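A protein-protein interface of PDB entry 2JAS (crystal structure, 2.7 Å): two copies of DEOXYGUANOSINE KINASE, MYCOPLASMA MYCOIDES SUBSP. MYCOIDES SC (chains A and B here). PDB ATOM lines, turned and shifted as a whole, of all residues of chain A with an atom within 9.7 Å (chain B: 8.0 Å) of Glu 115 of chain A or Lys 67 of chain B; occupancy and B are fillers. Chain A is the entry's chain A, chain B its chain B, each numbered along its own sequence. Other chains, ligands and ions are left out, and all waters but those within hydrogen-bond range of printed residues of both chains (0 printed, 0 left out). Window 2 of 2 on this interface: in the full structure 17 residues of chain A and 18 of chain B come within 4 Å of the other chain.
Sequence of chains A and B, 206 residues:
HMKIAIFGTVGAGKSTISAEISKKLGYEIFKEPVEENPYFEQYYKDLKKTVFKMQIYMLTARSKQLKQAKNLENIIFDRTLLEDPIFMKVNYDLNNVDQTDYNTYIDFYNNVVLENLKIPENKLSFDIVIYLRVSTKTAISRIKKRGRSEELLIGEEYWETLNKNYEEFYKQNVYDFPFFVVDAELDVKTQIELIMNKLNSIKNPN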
ATOM      1  N   SER A  63     -10.671 -13.313  -3.009  1.00  0.00           N
ATOM      2  CA  SER A  63     -10.632 -14.758  -2.871  1.00  0.00           C
ATOM      3  C   SER A  63      -9.670 -15.205  -1.762  1.00  0.00           C
ATOM      4  O   SER A  63      -9.902 -16.224  -1.110  1.00  0.00           O
ATOM      5  CB  SER A  63     -10.266 -15.385  -4.214  1.00  0.00           C
ATOM      6  OG  SER A  63      -9.700 -16.665  -4.035  1.00  0.00           O
ATOM      7  N   LEU A  66     -11.436 -14.319   1.589  1.00  0.00           N
ATOM      8  CA  LEU A  66     -12.412 -15.368   1.843  1.00  0.00           C
ATOM      9  C   LEU A  66     -11.692 -16.549   2.461  1.00  0.00           C
ATOM     10  O   LEU A  66     -12.055 -17.011   3.539  1.00  0.00           O
ATOM     11  CB  LEU A  66     -13.119 -15.799   0.555  1.00  0.00           C
ATOM     12  CG  LEU A  66     -14.178 -16.906   0.657  1.00  0.00           C
ATOM     13  CD1 LEU A  66     -15.389 -16.444   1.464  1.00  0.00           C
ATOM     14  CD2 LEU A  66     -14.612 -17.386  -0.725  1.00  0.00           C
ATOM     15  N   LYS A  67     -10.639 -16.996   1.782  1.00  0.00           N
ATOM     16  CA  LYS A  67      -9.856 -18.148   2.207  1.00  0.00           C
ATOM     17  C   LYS A  67      -8.944 -17.871   3.414  1.00  0.00           C
ATOM     18  O   LYS A  67      -7.891 -18.500   3.562  1.00  0.00           O
ATOM     19  CB  LYS A  67      -9.046 -18.698   1.027  1.00  0.00           C
ATOM     20  CG  LYS A  67      -9.905 -19.292  -0.090  1.00  0.00           C
ATOM     21  CD  LYS A  67      -9.049 -19.814  -1.244  1.00  0.00           C
ATOM     22  CE  LYS A  67      -9.913 -20.167  -2.440  1.00  0.00           C
ATOM     23  NZ  LYS A  67      -9.103 -20.237  -3.685  1.00  0.00           N
ATOM     24  N   LEU A  82     -18.508  -9.189  -3.217  1.00  0.00           N
ATOM     25  CA  LEU A  82     -19.446  -9.171  -4.337  1.00  0.00           C
ATOM     26  C   LEU A  82     -19.697  -7.769  -4.883  1.00  0.00           C
ATOM     27  O   LEU A  82     -20.701  -7.544  -5.561  1.00  0.00           O
ATOM     28  CB  LEU A  82     -20.786  -9.800  -3.926  1.00  0.00           C
ATOM     29  CG  LEU A  82     -20.817 -11.231  -3.376  1.00  0.00           C
ATOM     30  CD1 LEU A  82     -22.175 -11.546  -2.774  1.00  0.00           C
ATOM     31  CD2 LEU A  82     -20.464 -12.256  -4.449  1.00  0.00           C
ATOM     32  N   ILE A 106     -18.636  -9.479 -16.791  1.00  0.00           N
ATOM     33  CA  ILE A 106     -19.731 -10.093 -16.037  1.00  0.00           C
ATOM     34  C   ILE A 106     -19.965 -11.549 -16.416  1.00  0.00           C
ATOM     35  O   ILE A 106     -20.233 -12.378 -15.546  1.00  0.00           O
ATOM     36  CB  ILE A 106     -21.027  -9.247 -16.081  1.00  0.00           C
ATOM     37  CG1 ILE A 106     -20.825  -7.995 -15.233  1.00  0.00           C
ATOM     38  CG2 ILE A 106     -22.231 -10.017 -15.503  1.00  0.00           C
ATOM     39  CD1 ILE A 106     -21.666  -6.884 -15.649  1.00  0.00           C
ATOM     40  N   ASP A 107     -19.821 -11.867 -17.702  1.00  0.00           N
ATOM     41  CA  ASP A 107     -19.944 -13.249 -18.146  1.00  0.00           C
ATOM     42  C   ASP A 107     -18.961 -14.127 -17.390  1.00  0.00           C
ATOM     43  O   ASP A 107     -19.289 -15.245 -16.993  1.00  0.00           O
ATOM     44  CB  ASP A 107     -19.746 -13.367 -19.651  1.00  0.00           C
ATOM     45  CG  ASP A 107     -20.262 -14.684 -20.205  1.00  0.00           C
ATOM     46  OD1 ASP A 107     -21.181 -15.270 -19.589  1.00  0.00           O
ATOM     47  OD2 ASP A 107     -19.741 -15.129 -21.259  1.00  0.00           O
ATOM     48  N   PHE A 108     -17.765 -13.590 -17.167  1.00  0.00           N
ATOM     49  CA  PHE A 108     -16.734 -14.266 -16.390  1.00  0.00           C
ATOM     50  C   PHE A 108     -17.083 -14.335 -14.907  1.00  0.00           C
ATOM     51  O   PHE A 108     -16.909 -15.375 -14.269  1.00  0.00           O
ATOM     52  CB  PHE A 108     -15.376 -13.574 -16.569  1.00  0.00           C
ATOM     53  CG  PHE A 108     -14.307 -14.121 -15.670  1.00  0.00           C
ATOM     54  CD1 PHE A 108     -13.587 -15.252 -16.037  1.00  0.00           C
ATOM     55  CD2 PHE A 108     -14.042 -13.520 -14.441  1.00  0.00           C
ATOM     56  CE1 PHE A 108     -12.610 -15.772 -15.206  1.00  0.00           C
ATOM     57  CE2 PHE A 108     -13.067 -14.033 -13.600  1.00  0.00           C
ATOM     58  CZ  PHE A 108     -12.352 -15.167 -13.985  1.00  0.00           C
ATOM     59  N   TYR A 109     -17.548 -13.217 -14.364  1.00  0.00           N
ATOM     60  CA  TYR A 109     -17.941 -13.141 -12.968  1.00  0.00           C
ATOM     61  C   TYR A 109     -19.000 -14.181 -12.612  1.00  0.00           C
ATOM     62  O   TYR A 109     -18.832 -14.931 -11.657  1.00  0.00           O
ATOM     63  CB  TYR A 109     -18.449 -11.741 -12.651  1.00  0.00           C
ATOM     64  CG  TYR A 109     -18.504 -11.418 -11.181  1.00  0.00           C
ATOM     65  CD1 TYR A 109     -17.398 -10.865 -10.528  1.00  0.00           C
ATOM     66  CD2 TYR A 109     -19.675 -11.634 -10.439  1.00  0.00           C
ATOM     67  CE1 TYR A 109     -17.446 -10.545  -9.176  1.00  0.00           C
ATOM     68  CE2 TYR A 109     -19.736 -11.316  -9.080  1.00  0.00           C
ATOM     69  CZ  TYR A 109     -18.616 -10.775  -8.457  1.00  0.00           C
ATOM     70  OH  TYR A 109     -18.666 -10.460  -7.115  1.00  0.00           O
ATOM     71  N   ASN A 110     -20.076 -14.235 -13.394  1.00  0.00           N
ATOM     72  CA  ASN A 110     -21.157 -15.190 -13.164  1.00  0.00           C
ATOM     73  C   ASN A 110     -20.687 -16.642 -13.180  1.00  0.00           C
ATOM     74  O   ASN A 110     -20.906 -17.385 -12.227  1.00  0.00           O
ATOM     75  CB  ASN A 110     -22.277 -15.005 -14.198  1.00  0.00           C
ATOM     76  CG  ASN A 110     -23.001 -13.668 -14.070  1.00  0.00           C
ATOM     77  OD1 ASN A 110     -23.615 -13.208 -15.028  1.00  0.00           O
ATOM     78  ND2 ASN A 110     -22.947 -13.054 -12.897  1.00  0.00           N
ATOM     79  N   ASN A 111     -20.042 -17.029 -14.274  1.00  0.00           N
ATOM     80  CA  ASN A 111     -19.611 -18.408 -14.502  1.00  0.00           C
ATOM     81  C   ASN A 111     -18.467 -18.909 -13.608  1.00  0.00           C
ATOM     82  O   ASN A 111     -18.404 -20.094 -13.276  1.00  0.00           O
ATOM     83  CB  ASN A 111     -19.254 -18.594 -15.978  1.00  0.00           C
ATOM     84  CG  ASN A 111     -20.481 -18.755 -16.855  1.00  0.00           C
ATOM     85  OD1 ASN A 111     -21.080 -19.829 -16.902  1.00  0.00           O
ATOM     86  ND2 ASN A 111     -20.851 -17.693 -17.568  1.00  0.00           N
ATOM     87  N   VAL A 112     -17.568 -18.006 -13.227  1.00  0.00           N
ATOM     88  CA  VAL A 112     -16.413 -18.369 -12.402  1.00  0.00           C
ATOM     89  C   VAL A 112     -16.578 -17.932 -10.932  1.00  0.00           C
ATOM     90  O   VAL A 112     -16.631 -18.775 -10.038  1.00  0.00           O
ATOM     91  CB  VAL A 112     -15.082 -17.859 -13.027  1.00  0.00           C
ATOM     92  CG1 VAL A 112     -13.879 -18.298 -12.205  1.00  0.00           C
ATOM     93  CG2 VAL A 112     -14.944 -18.362 -14.450  1.00  0.00           C
ATOM     94  N   VAL A 113     -16.679 -16.631 -10.682  1.00  0.00           N
ATOM     95  CA  VAL A 113     -16.706 -16.130  -9.299  1.00  0.00           C
ATOM     96  C   VAL A 113     -17.951 -16.584  -8.526  1.00  0.00           C
ATOM     97  O   VAL A 113     -17.833 -17.184  -7.455  1.00  0.00           O
ATOM     98  CB  VAL A 113     -16.564 -14.587  -9.220  1.00  0.00           C
ATOM     99  CG1 VAL A 113     -16.590 -14.123  -7.767  1.00  0.00           C
ATOM    100  CG2 VAL A 113     -15.283 -14.122  -9.902  1.00  0.00           C
ATOM    101  N   LEU A 114     -19.134 -16.312  -9.078  1.00  0.00           N
ATOM    102  CA  LEU A 114     -20.388 -16.595  -8.383  1.00  0.00           C
ATOM    103  C   LEU A 114     -20.630 -18.079  -8.097  1.00  0.00           C
ATOM    104  O   LEU A 114     -21.300 -18.419  -7.121  1.00  0.00           O
ATOM    105  CB  LEU A 114     -21.578 -15.964  -9.113  1.00  0.00           C
ATOM    106  CG  LEU A 114     -21.842 -14.483  -8.811  1.00  0.00           C
ATOM    107  CD1 LEU A 114     -22.990 -13.946  -9.659  1.00  0.00           C
ATOM    108  CD2 LEU A 114     -22.125 -14.250  -7.320  1.00  0.00           C
ATOM    109  N   GLU A 115     -20.084 -18.954  -8.940  1.00  0.00           N
ATOM    110  CA  GLU A 115     -20.072 -20.388  -8.657  1.00  0.00           C
ATOM    111  C   GLU A 115     -19.018 -20.656  -7.583  1.00  0.00           C
ATOM    112  O   GLU A 115     -17.852 -20.263  -7.732  1.00  0.00           O
ATOM    113  CB  GLU A 115     -19.758 -21.193  -9.921  1.00  0.00           C
ATOM    114  CG  GLU A 115     -20.620 -20.852 -11.147  1.00  0.00           C
ATOM    115  CD  GLU A 115     -21.957 -21.581 -11.181  1.00  0.00           C
ATOM    116  OE1 GLU A 115     -22.724 -21.493 -10.195  1.00  0.00           O
ATOM    117  OE2 GLU A 115     -22.250 -22.227 -12.210  1.00  0.00           O
ATOM    118  N   ASN A 116     -19.442 -21.298  -6.491  1.00  0.00           N
ATOM    119  CA  ASN A 116     -18.571 -21.561  -5.324  1.00  0.00           C
ATOM    120  C   ASN A 116     -19.039 -22.708  -4.395  1.00  0.00           C
ATOM    121  O   ASN A 116     -20.229 -22.848  -4.067  1.00  0.00           O
ATOM    122  CB  ASN A 116     -18.328 -20.272  -4.524  1.00  0.00           C
ATOM    123  CG  ASN A 116     -19.613 -19.520  -4.214  1.00  0.00           C
ATOM    124  OD1 ASN A 116     -20.647 -20.124  -3.910  1.00  0.00           O
ATOM    125  ND2 ASN A 116     -19.552 -18.190  -4.283  1.00  0.00           N
ATOM    126  N   LYS A 123     -17.979 -20.126   1.308  1.00  0.00           N
ATOM    127  CA  LYS A 123     -19.074 -19.154   1.206  1.00  0.00           C
ATOM    128  C   LYS A 123     -19.374 -18.439   2.540  1.00  0.00           C
ATOM    129  O   LYS A 123     -19.624 -19.087   3.569  1.00  0.00           O
ATOM    130  CB  LYS A 123     -20.346 -19.833   0.679  1.00  0.00           C
ATOM    131  CG  LYS A 123     -21.510 -18.877   0.416  1.00  0.00           C
ATOM    132  CD  LYS A 123     -22.839 -19.460   0.900  1.00  0.00           C
ATOM    133  CE  LYS A 123     -23.935 -18.396   0.879  1.00  0.00           C
ATOM    134  NZ  LYS A 123     -24.885 -18.525   2.029  1.00  0.00           N
ATOM    135  N   TYR A 175     -28.172  -9.903  -4.226  1.00  0.00           N
ATOM    136  CA  TYR A 175     -27.735 -11.032  -3.405  1.00  0.00           C
ATOM    137  C   TYR A 175     -28.538 -11.195  -2.117  1.00  0.00           C
ATOM    138  O   TYR A 175     -28.250 -12.084  -1.314  1.00  0.00           O
ATOM    139  CB  TYR A 175     -26.222 -10.960  -3.151  1.00  0.00           C
ATOM    140  CG  TYR A 175     -25.435 -10.806  -4.446  1.00  0.00           C
ATOM    141  CD1 TYR A 175     -24.686  -9.652  -4.702  1.00  0.00           C
ATOM    142  CD2 TYR A 175     -25.479 -11.793  -5.429  1.00  0.00           C
ATOM    143  CE1 TYR A 175     -23.995  -9.499  -5.889  1.00  0.00           C
ATOM    144  CE2 TYR A 175     -24.790 -11.648  -6.622  1.00  0.00           C
ATOM    145  CZ  TYR A 175     -24.052 -10.503  -6.846  1.00  0.00           C
ATOM    146  OH  TYR A 175     -23.373 -10.366  -8.028  1.00  0.00           O
ATOM    147  N   PHE B  30     -15.575 -30.774 -29.360  1.00  0.00           N
ATOM    148  CA  PHE B  30     -15.757 -29.543 -28.593  1.00  0.00           C
ATOM    149  C   PHE B  30     -14.734 -28.495 -29.013  1.00  0.00           C
ATOM    150  O   PHE B  30     -13.530 -28.725 -28.929  1.00  0.00           O
ATOM    151  CB  PHE B  30     -15.665 -29.829 -27.093  1.00  0.00           C
ATOM    152  CG  PHE B  30     -16.929 -30.394 -26.510  1.00  0.00           C
ATOM    153  CD1 PHE B  30     -17.260 -31.733 -26.689  1.00  0.00           C
ATOM    154  CD2 PHE B  30     -17.798 -29.582 -25.791  1.00  0.00           C
ATOM    155  CE1 PHE B  30     -18.437 -32.256 -26.157  1.00  0.00           C
ATOM    156  CE2 PHE B  30     -18.977 -30.097 -25.251  1.00  0.00           C
ATOM    157  CZ  PHE B  30     -19.296 -31.436 -25.437  1.00  0.00           C
ATOM    158  N   ALA B  61     -14.965 -19.247 -21.458  1.00  0.00           N
ATOM    159  CA  ALA B  61     -15.358 -20.291 -22.412  1.00  0.00           C
ATOM    160  C   ALA B  61     -14.975 -21.702 -21.940  1.00  0.00           C
ATOM    161  O   ALA B  61     -15.776 -22.628 -22.077  1.00  0.00           O
ATOM    162  CB  ALA B  61     -14.802 -19.996 -23.784  1.00  0.00           C
ATOM    163  N   ARG B  62     -13.771 -21.846 -21.371  1.00  0.00           N
ATOM    164  CA  ARG B  62     -13.316 -23.111 -20.764  1.00  0.00           C
ATOM    165  C   ARG B  62     -14.278 -23.567 -19.671  1.00  0.00           C
ATOM    166  O   ARG B  62     -14.735 -24.711 -19.660  1.00  0.00           O
ATOM    167  CB  ARG B  62     -11.908 -22.986 -20.143  1.00  0.00           C
ATOM    168  CG  ARG B  62     -10.834 -22.303 -20.977  1.00  0.00           C
ATOM    169  CD  ARG B  62     -10.502 -23.048 -22.250  1.00  0.00           C
ATOM    170  NE  ARG B  62      -9.619 -22.258 -23.094  1.00  0.00           N
ATOM    171  CZ  ARG B  62      -9.639 -22.280 -24.421  1.00  0.00           C
ATOM    172  NH1 ARG B  62     -10.507 -23.051 -25.063  1.00  0.00           N
ATOM    173  NH2 ARG B  62      -8.795 -21.528 -25.114  1.00  0.00           N
ATOM    174  N   SER B  63     -14.562 -22.653 -18.748  1.00  0.00           N
ATOM    175  CA  SER B  63     -15.515 -22.867 -17.672  1.00  0.00           C
ATOM    176  C   SER B  63     -16.876 -23.394 -18.161  1.00  0.00           C
ATOM    177  O   SER B  63     -17.483 -24.249 -17.518  1.00  0.00           O
ATOM    178  CB  SER B  63     -15.666 -21.562 -16.883  1.00  0.00           C
ATOM    179  OG  SER B  63     -16.911 -21.482 -16.218  1.00  0.00           O
ATOM    180  N   LYS B  64     -17.346 -22.891 -19.298  1.00  0.00           N
ATOM    181  CA  LYS B  64     -18.610 -23.351 -19.883  1.00  0.00           C
ATOM    182  C   LYS B  64     -18.493 -24.768 -20.447  1.00  0.00           C
ATOM    183  O   LYS B  64     -19.343 -25.623 -20.178  1.00  0.00           O
ATOM    184  CB  LYS B  64     -19.104 -22.381 -20.964  1.00  0.00           C
ATOM    185  CG  LYS B  64     -19.645 -21.075 -20.414  1.00  0.00           C
ATOM    186  CD  LYS B  64     -19.719 -20.006 -21.485  1.00  0.00           C
ATOM    187  CE  LYS B  64     -20.230 -18.705 -20.882  1.00  0.00           C
ATOM    188  NZ  LYS B  64     -20.634 -17.704 -21.912  1.00  0.00           N
ATOM    189  N   GLN B  65     -17.439 -25.014 -21.220  1.00  0.00           N
ATOM    190  CA  GLN B  65     -17.220 -26.332 -21.809  1.00  0.00           C
ATOM    191  C   GLN B  65     -17.173 -27.431 -20.748  1.00  0.00           C
ATOM    192  O   GLN B  65     -17.739 -28.506 -20.940  1.00  0.00           O
ATOM    193  CB  GLN B  65     -15.956 -26.347 -22.666  1.00  0.00           C
ATOM    194  CG  GLN B  65     -16.124 -25.678 -24.018  1.00  0.00           C
ATOM    195  CD  GLN B  65     -14.840 -25.646 -24.813  1.00  0.00           C
ATOM    196  OE1 GLN B  65     -13.746 -25.710 -24.254  1.00  0.00           O
ATOM    197  NE2 GLN B  65     -14.965 -25.538 -26.132  1.00  0.00           N
ATOM    198  N   LEU B  66     -16.517 -27.151 -19.628  1.00  0.00           N
ATOM    199  CA  LEU B  66     -16.464 -28.100 -18.517  1.00  0.00           C
ATOM    200  C   LEU B  66     -17.858 -28.479 -18.011  1.00  0.00           C
ATOM    201  O   LEU B  66     -18.110 -29.643 -17.696  1.00  0.00           O
ATOM    202  CB  LEU B  66     -15.617 -27.550 -17.365  1.00  0.00           C
ATOM    203  CG  LEU B  66     -15.408 -28.452 -16.140  1.00  0.00           C
ATOM    204  CD1 LEU B  66     -14.497 -29.632 -16.456  1.00  0.00           C
ATOM    205  CD2 LEU B  66     -14.845 -27.657 -14.979  1.00  0.00           C
ATOM    206  N   LYS B  67     -18.752 -27.496 -17.937  1.00  0.00           N
ATOM    207  CA  LYS B  67     -20.108 -27.721 -17.445  1.00  0.00           C
ATOM    208  C   LYS B  67     -20.827 -28.839 -18.204  1.00  0.00           C
ATOM    209  O   LYS B  67     -21.483 -29.689 -17.598  1.00  0.00           O
ATOM    210  CB  LYS B  67     -20.931 -26.431 -17.500  1.00  0.00           C
ATOM    211  CG  LYS B  67     -20.910 -25.609 -16.225  1.00  0.00           C
ATOM    212  CD  LYS B  67     -22.031 -24.582 -16.248  1.00  0.00           C
ATOM    213  CE  LYS B  67     -22.570 -24.313 -14.853  1.00  0.00           C
ATOM    214  NZ  LYS B  67     -23.991 -23.854 -14.905  1.00  0.00           N
ATOM    215  N   GLN B  68     -20.688 -28.838 -19.525  1.00  0.00           N
ATOM    216  CA  GLN B  68     -21.360 -29.822 -20.369  1.00  0.00           C
ATOM    217  C   GLN B  68     -20.570 -31.129 -20.507  1.00  0.00           C
ATOM    218  O   GLN B  68     -21.154 -32.212 -20.481  1.00  0.00           O
ATOM    219  CB  GLN B  68     -21.700 -29.212 -21.737  1.00  0.00           C
ATOM    220  CG  GLN B  68     -20.550 -28.456 -22.395  1.00  0.00           C
ATOM    221  CD  GLN B  68     -20.956 -27.106 -22.973  1.00  0.00           C
ATOM    222  OE1 GLN B  68     -22.012 -26.563 -22.647  1.00  0.00           O
ATOM    223  NE2 GLN B  68     -20.102 -26.551 -23.830  1.00  0.00           N
ATOM    224  N   ALA B  69     -19.248 -31.018 -20.622  1.00  0.00           N
ATOM    225  CA  ALA B  69     -18.377 -32.165 -20.896  1.00  0.00           C
ATOM    226  C   ALA B  69     -18.319 -33.239 -19.799  1.00  0.00           C
ATOM    227  O   ALA B  69     -18.337 -34.433 -20.108  1.00  0.00           O
ATOM    228  CB  ALA B  69     -16.972 -31.691 -21.247  1.00  0.00           C
ATOM    229  N   LYS B  70     -18.290 -32.822 -18.535  1.00  0.00           N
ATOM    230  CA  LYS B  70     -18.064 -33.750 -17.425  1.00  0.00           C
ATOM    231  C   LYS B  70     -19.301 -34.579 -17.062  1.00  0.00           C
ATOM    232  O   LYS B  70     -19.415 -35.085 -15.945  1.00  0.00           O
ATOM    233  CB  LYS B  70     -17.554 -32.999 -16.195  1.00  0.00           C
ATOM    234  CG  LYS B  70     -16.039 -32.916 -16.101  1.00  0.00           C
ATOM    235  CD  LYS B  70     -15.580 -32.804 -14.657  1.00  0.00           C
ATOM    236  CE  LYS B  70     -14.076 -32.986 -14.540  1.00  0.00           C
ATOM    237  NZ  LYS B  70     -13.554 -32.476 -13.242  1.00  0.00           N
ATOM    238  N   ASN B  71     -20.219 -34.711 -18.013  1.00  0.00           N
ATOM    239  CA  ASN B  71     -21.327 -35.656 -17.930  1.00  0.00           C
ATOM    240  C   ASN B  71     -21.547 -36.392 -19.252  1.00  0.00           C
ATOM    241  O   ASN B  71     -22.670 -36.762 -19.598  1.00  0.00           O
ATOM    242  CB  ASN B  71     -22.602 -34.957 -17.460  1.00  0.00           C
ATOM    243  CG  ASN B  71     -22.611 -34.717 -15.968  1.00  0.00           C
ATOM    244  OD1 ASN B  71     -21.970 -33.789 -15.472  1.00  0.00           O
ATOM    245  ND2 ASN B  71     -23.339 -35.556 -15.240  1.00  0.00           N
ATOM    246  N   LEU B  72     -20.453 -36.604 -19.980  1.00  0.00           N
ATOM    247  CA  LEU B  72     -20.485 -37.282 -21.270  1.00  0.00           C
ATOM    248  C   LEU B  72     -19.360 -38.305 -21.354  1.00  0.00           C
ATOM    249  O   LEU B  72     -18.225 -38.027 -20.965  1.00  0.00           O
ATOM    250  CB  LEU B  72     -20.378 -36.272 -22.421  1.00  0.00           C
ATOM    251  CG  LEU B  72     -21.483 -35.221 -22.607  1.00  0.00           C
ATOM    252  CD1 LEU B  72     -21.102 -34.221 -23.687  1.00  0.00           C
ATOM    253  CD2 LEU B  72     -22.841 -35.854 -22.919  1.00  0.00           C
ATOM    254  N   PHE B  77     -11.870 -33.444 -27.743  1.00  0.00           N
ATOM    255  CA  PHE B  77     -11.551 -32.066 -27.392  1.00  0.00           C
ATOM    256  C   PHE B  77     -10.420 -31.531 -28.249  1.00  0.00           C
ATOM    257  O   PHE B  77      -9.320 -32.082 -28.250  1.00  0.00           O
ATOM    258  CB  PHE B  77     -11.150 -31.962 -25.916  1.00  0.00           C
ATOM    259  CG  PHE B  77     -12.186 -31.323 -25.030  1.00  0.00           C
ATOM    260  CD1 PHE B  77     -13.221 -32.075 -24.490  1.00  0.00           C
ATOM    261  CD2 PHE B  77     -12.096 -29.974 -24.699  1.00  0.00           C
ATOM    262  CE1 PHE B  77     -14.164 -31.489 -23.651  1.00  0.00           C
ATOM    263  CE2 PHE B  77     -13.035 -29.379 -23.859  1.00  0.00           C
ATOM    264  CZ  PHE B  77     -14.071 -30.140 -23.335  1.00  0.00           C
ATOM    265  N   LEU B  81      -8.652 -27.614 -21.186  1.00  0.00           N
ATOM    266  CA  LEU B  81      -9.095 -26.425 -20.474  1.00  0.00           C
ATOM    267  C   LEU B  81      -7.955 -25.693 -19.761  1.00  0.00           C
ATOM    268  O   LEU B  81      -8.134 -24.562 -19.273  1.00  0.00           O
ATOM    269  CB  LEU B  81     -10.171 -26.810 -19.466  1.00  0.00           C
ATOM    270  CG  LEU B  81     -11.162 -27.864 -19.950  1.00  0.00           C
ATOM    271  CD1 LEU B  81     -11.940 -28.416 -18.768  1.00  0.00           C
ATOM    272  CD2 LEU B  81     -12.091 -27.305 -21.026  1.00  0.00           C
ATOM    273  N   VAL B 112      -8.357 -18.406  -8.162  1.00  0.00           N
ATOM    274  CA  VAL B 112      -9.726 -18.188  -8.629  1.00  0.00           C
ATOM    275  C   VAL B 112     -10.158 -19.232  -9.673  1.00  0.00           C
ATOM    276  O   VAL B 112     -11.144 -19.935  -9.454  1.00  0.00           O
ATOM    277  CB  VAL B 112      -9.953 -16.738  -9.138  1.00  0.00           C
ATOM    278  CG1 VAL B 112     -11.381 -16.547  -9.613  1.00  0.00           C
ATOM    279  CG2 VAL B 112      -9.640 -15.745  -8.044  1.00  0.00           C
ATOM    280  N   GLU B 115     -10.520 -23.386  -9.047  1.00  0.00           N
ATOM    281  CA  GLU B 115     -11.538 -23.803  -8.085  1.00  0.00           C
ATOM    282  C   GLU B 115     -12.664 -24.597  -8.753  1.00  0.00           C
ATOM    283  O   GLU B 115     -13.582 -25.060  -8.083  1.00  0.00           O
ATOM    284  CB  GLU B 115     -12.087 -22.594  -7.336  1.00  0.00           C
ATOM    285  CG  GLU B 115     -11.090 -21.991  -6.359  1.00  0.00           C
ATOM    286  CD  GLU B 115     -11.123 -22.651  -4.987  1.00  0.00           C
ATOM    287  OE1 GLU B 115     -12.080 -22.385  -4.231  1.00  0.00           O
ATOM    288  OE2 GLU B 115     -10.189 -23.419  -4.662  1.00  0.00           O
ATOM    289  N   ASN B 116     -12.579 -24.761 -10.074  1.00  0.00           N
ATOM    290  CA  ASN B 116     -13.466 -25.675 -10.801  1.00  0.00           C
ATOM    291  C   ASN B 116     -13.238 -27.154 -10.431  1.00  0.00           C
ATOM    292  O   ASN B 116     -14.156 -27.974 -10.529  1.00  0.00           O
ATOM    293  CB  ASN B 116     -13.368 -25.456 -12.323  1.00  0.00           C
ATOM    294  CG  ASN B 116     -12.005 -25.863 -12.917  1.00  0.00           C
ATOM    295  OD1 ASN B 116     -11.400 -26.867 -12.524  1.00  0.00           O
ATOM    296  ND2 ASN B 116     -11.540 -25.090 -13.902  1.00  0.00           N
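The side-chain amide nitrogen (ND2) of Asn 111 of chain A lies within hydrogen-bond range of the backbone carbonyl oxygen (O) of Asp 107 of chain A.
Glu 115 of chain A touches just one residue of chain B: Lys 67. Of chain A, only Glu 115 comes within 4 Å of Lys 67 of chain B. No residue of chain A comes within 4 Å of Leu 66 of chain B. Of the printed residues of chain B, Lys 67 of chain A touches Glu 115 (3.4 Å). Printed residues of chain A within 4 Å of Val 112 of chain B: Ser 63 (3.9 Å). Printed residues of chain A within 4 Å of Glu 115 of chain B: Lys 67. Of the printed residues of chain B, Asp 107 of chain A touches Lys 64. Phe 77 of chain B touches none of the printed residues of chain A. The nearest residue of chain A that does not touch Lys 67 of chain B is Asn 111 of chain A (4.9 Å). The nearest printed residue of chain A that does not touch Lys 64 of chain B is Phe 108 of chain A (6.8 Å).
Among the printed residues, merely in contact across the chains: Asn 111 of chain A with Lys 64 of chain B, Asn 111 of chain A with Ser 63 of chain B and Ser 63 of chain A with Val 112 of chain B.
Ser 63 of chain A touches Val 112 of chain B, but with the chains exchanged Val 112 of chain A does not touch Ser 63 of chain B (4.1 Å). Lys 67 of chain A touches Glu 115 of chain B, and with the chains exchanged Glu 115 of chain A touches Lys 67 of chain B. Of the 6 pairs that touch across the chains among the printed residues, 2 have their exchanged pair printed and touching as well.
Printed residues of chain A that touch a printed residue of chain B: Ser 63, Lys 67, Asp 107, Asn 111 and Glu 115. Hydrophobic or aromatic side chains of chain B that line the printed part of chain A: Val 112. Among the printed residues, Asp or Glu carboxylates within 4 Å of a Lys or Arg side-chain nitrogen of the other chain: Lys 67 of chain A with Glu 115 of chain B (3.5 Å), Asp 107 of chain A with Lys 64 of chain B (2.8 Å) and Glu 115 of chain A with Lys 67 of chain B (3.6 Å).
NZ of Lys 64 of chain B is in salt-bridge range of OD2 of Asp 107 of chain A. The side-chain amino group (NZ) of Lys 67 of chain A lies within salt-bridge range of the side-chain carboxylate (OE2) of Glu 115 of chain B, 3.5 Å away. The side-chain amino group (NZ) of Lys 67 of chain B lies within salt-bridge range of the side-chain carboxylate (OE2) of Glu 115 of chain A, at 3.6 Å.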
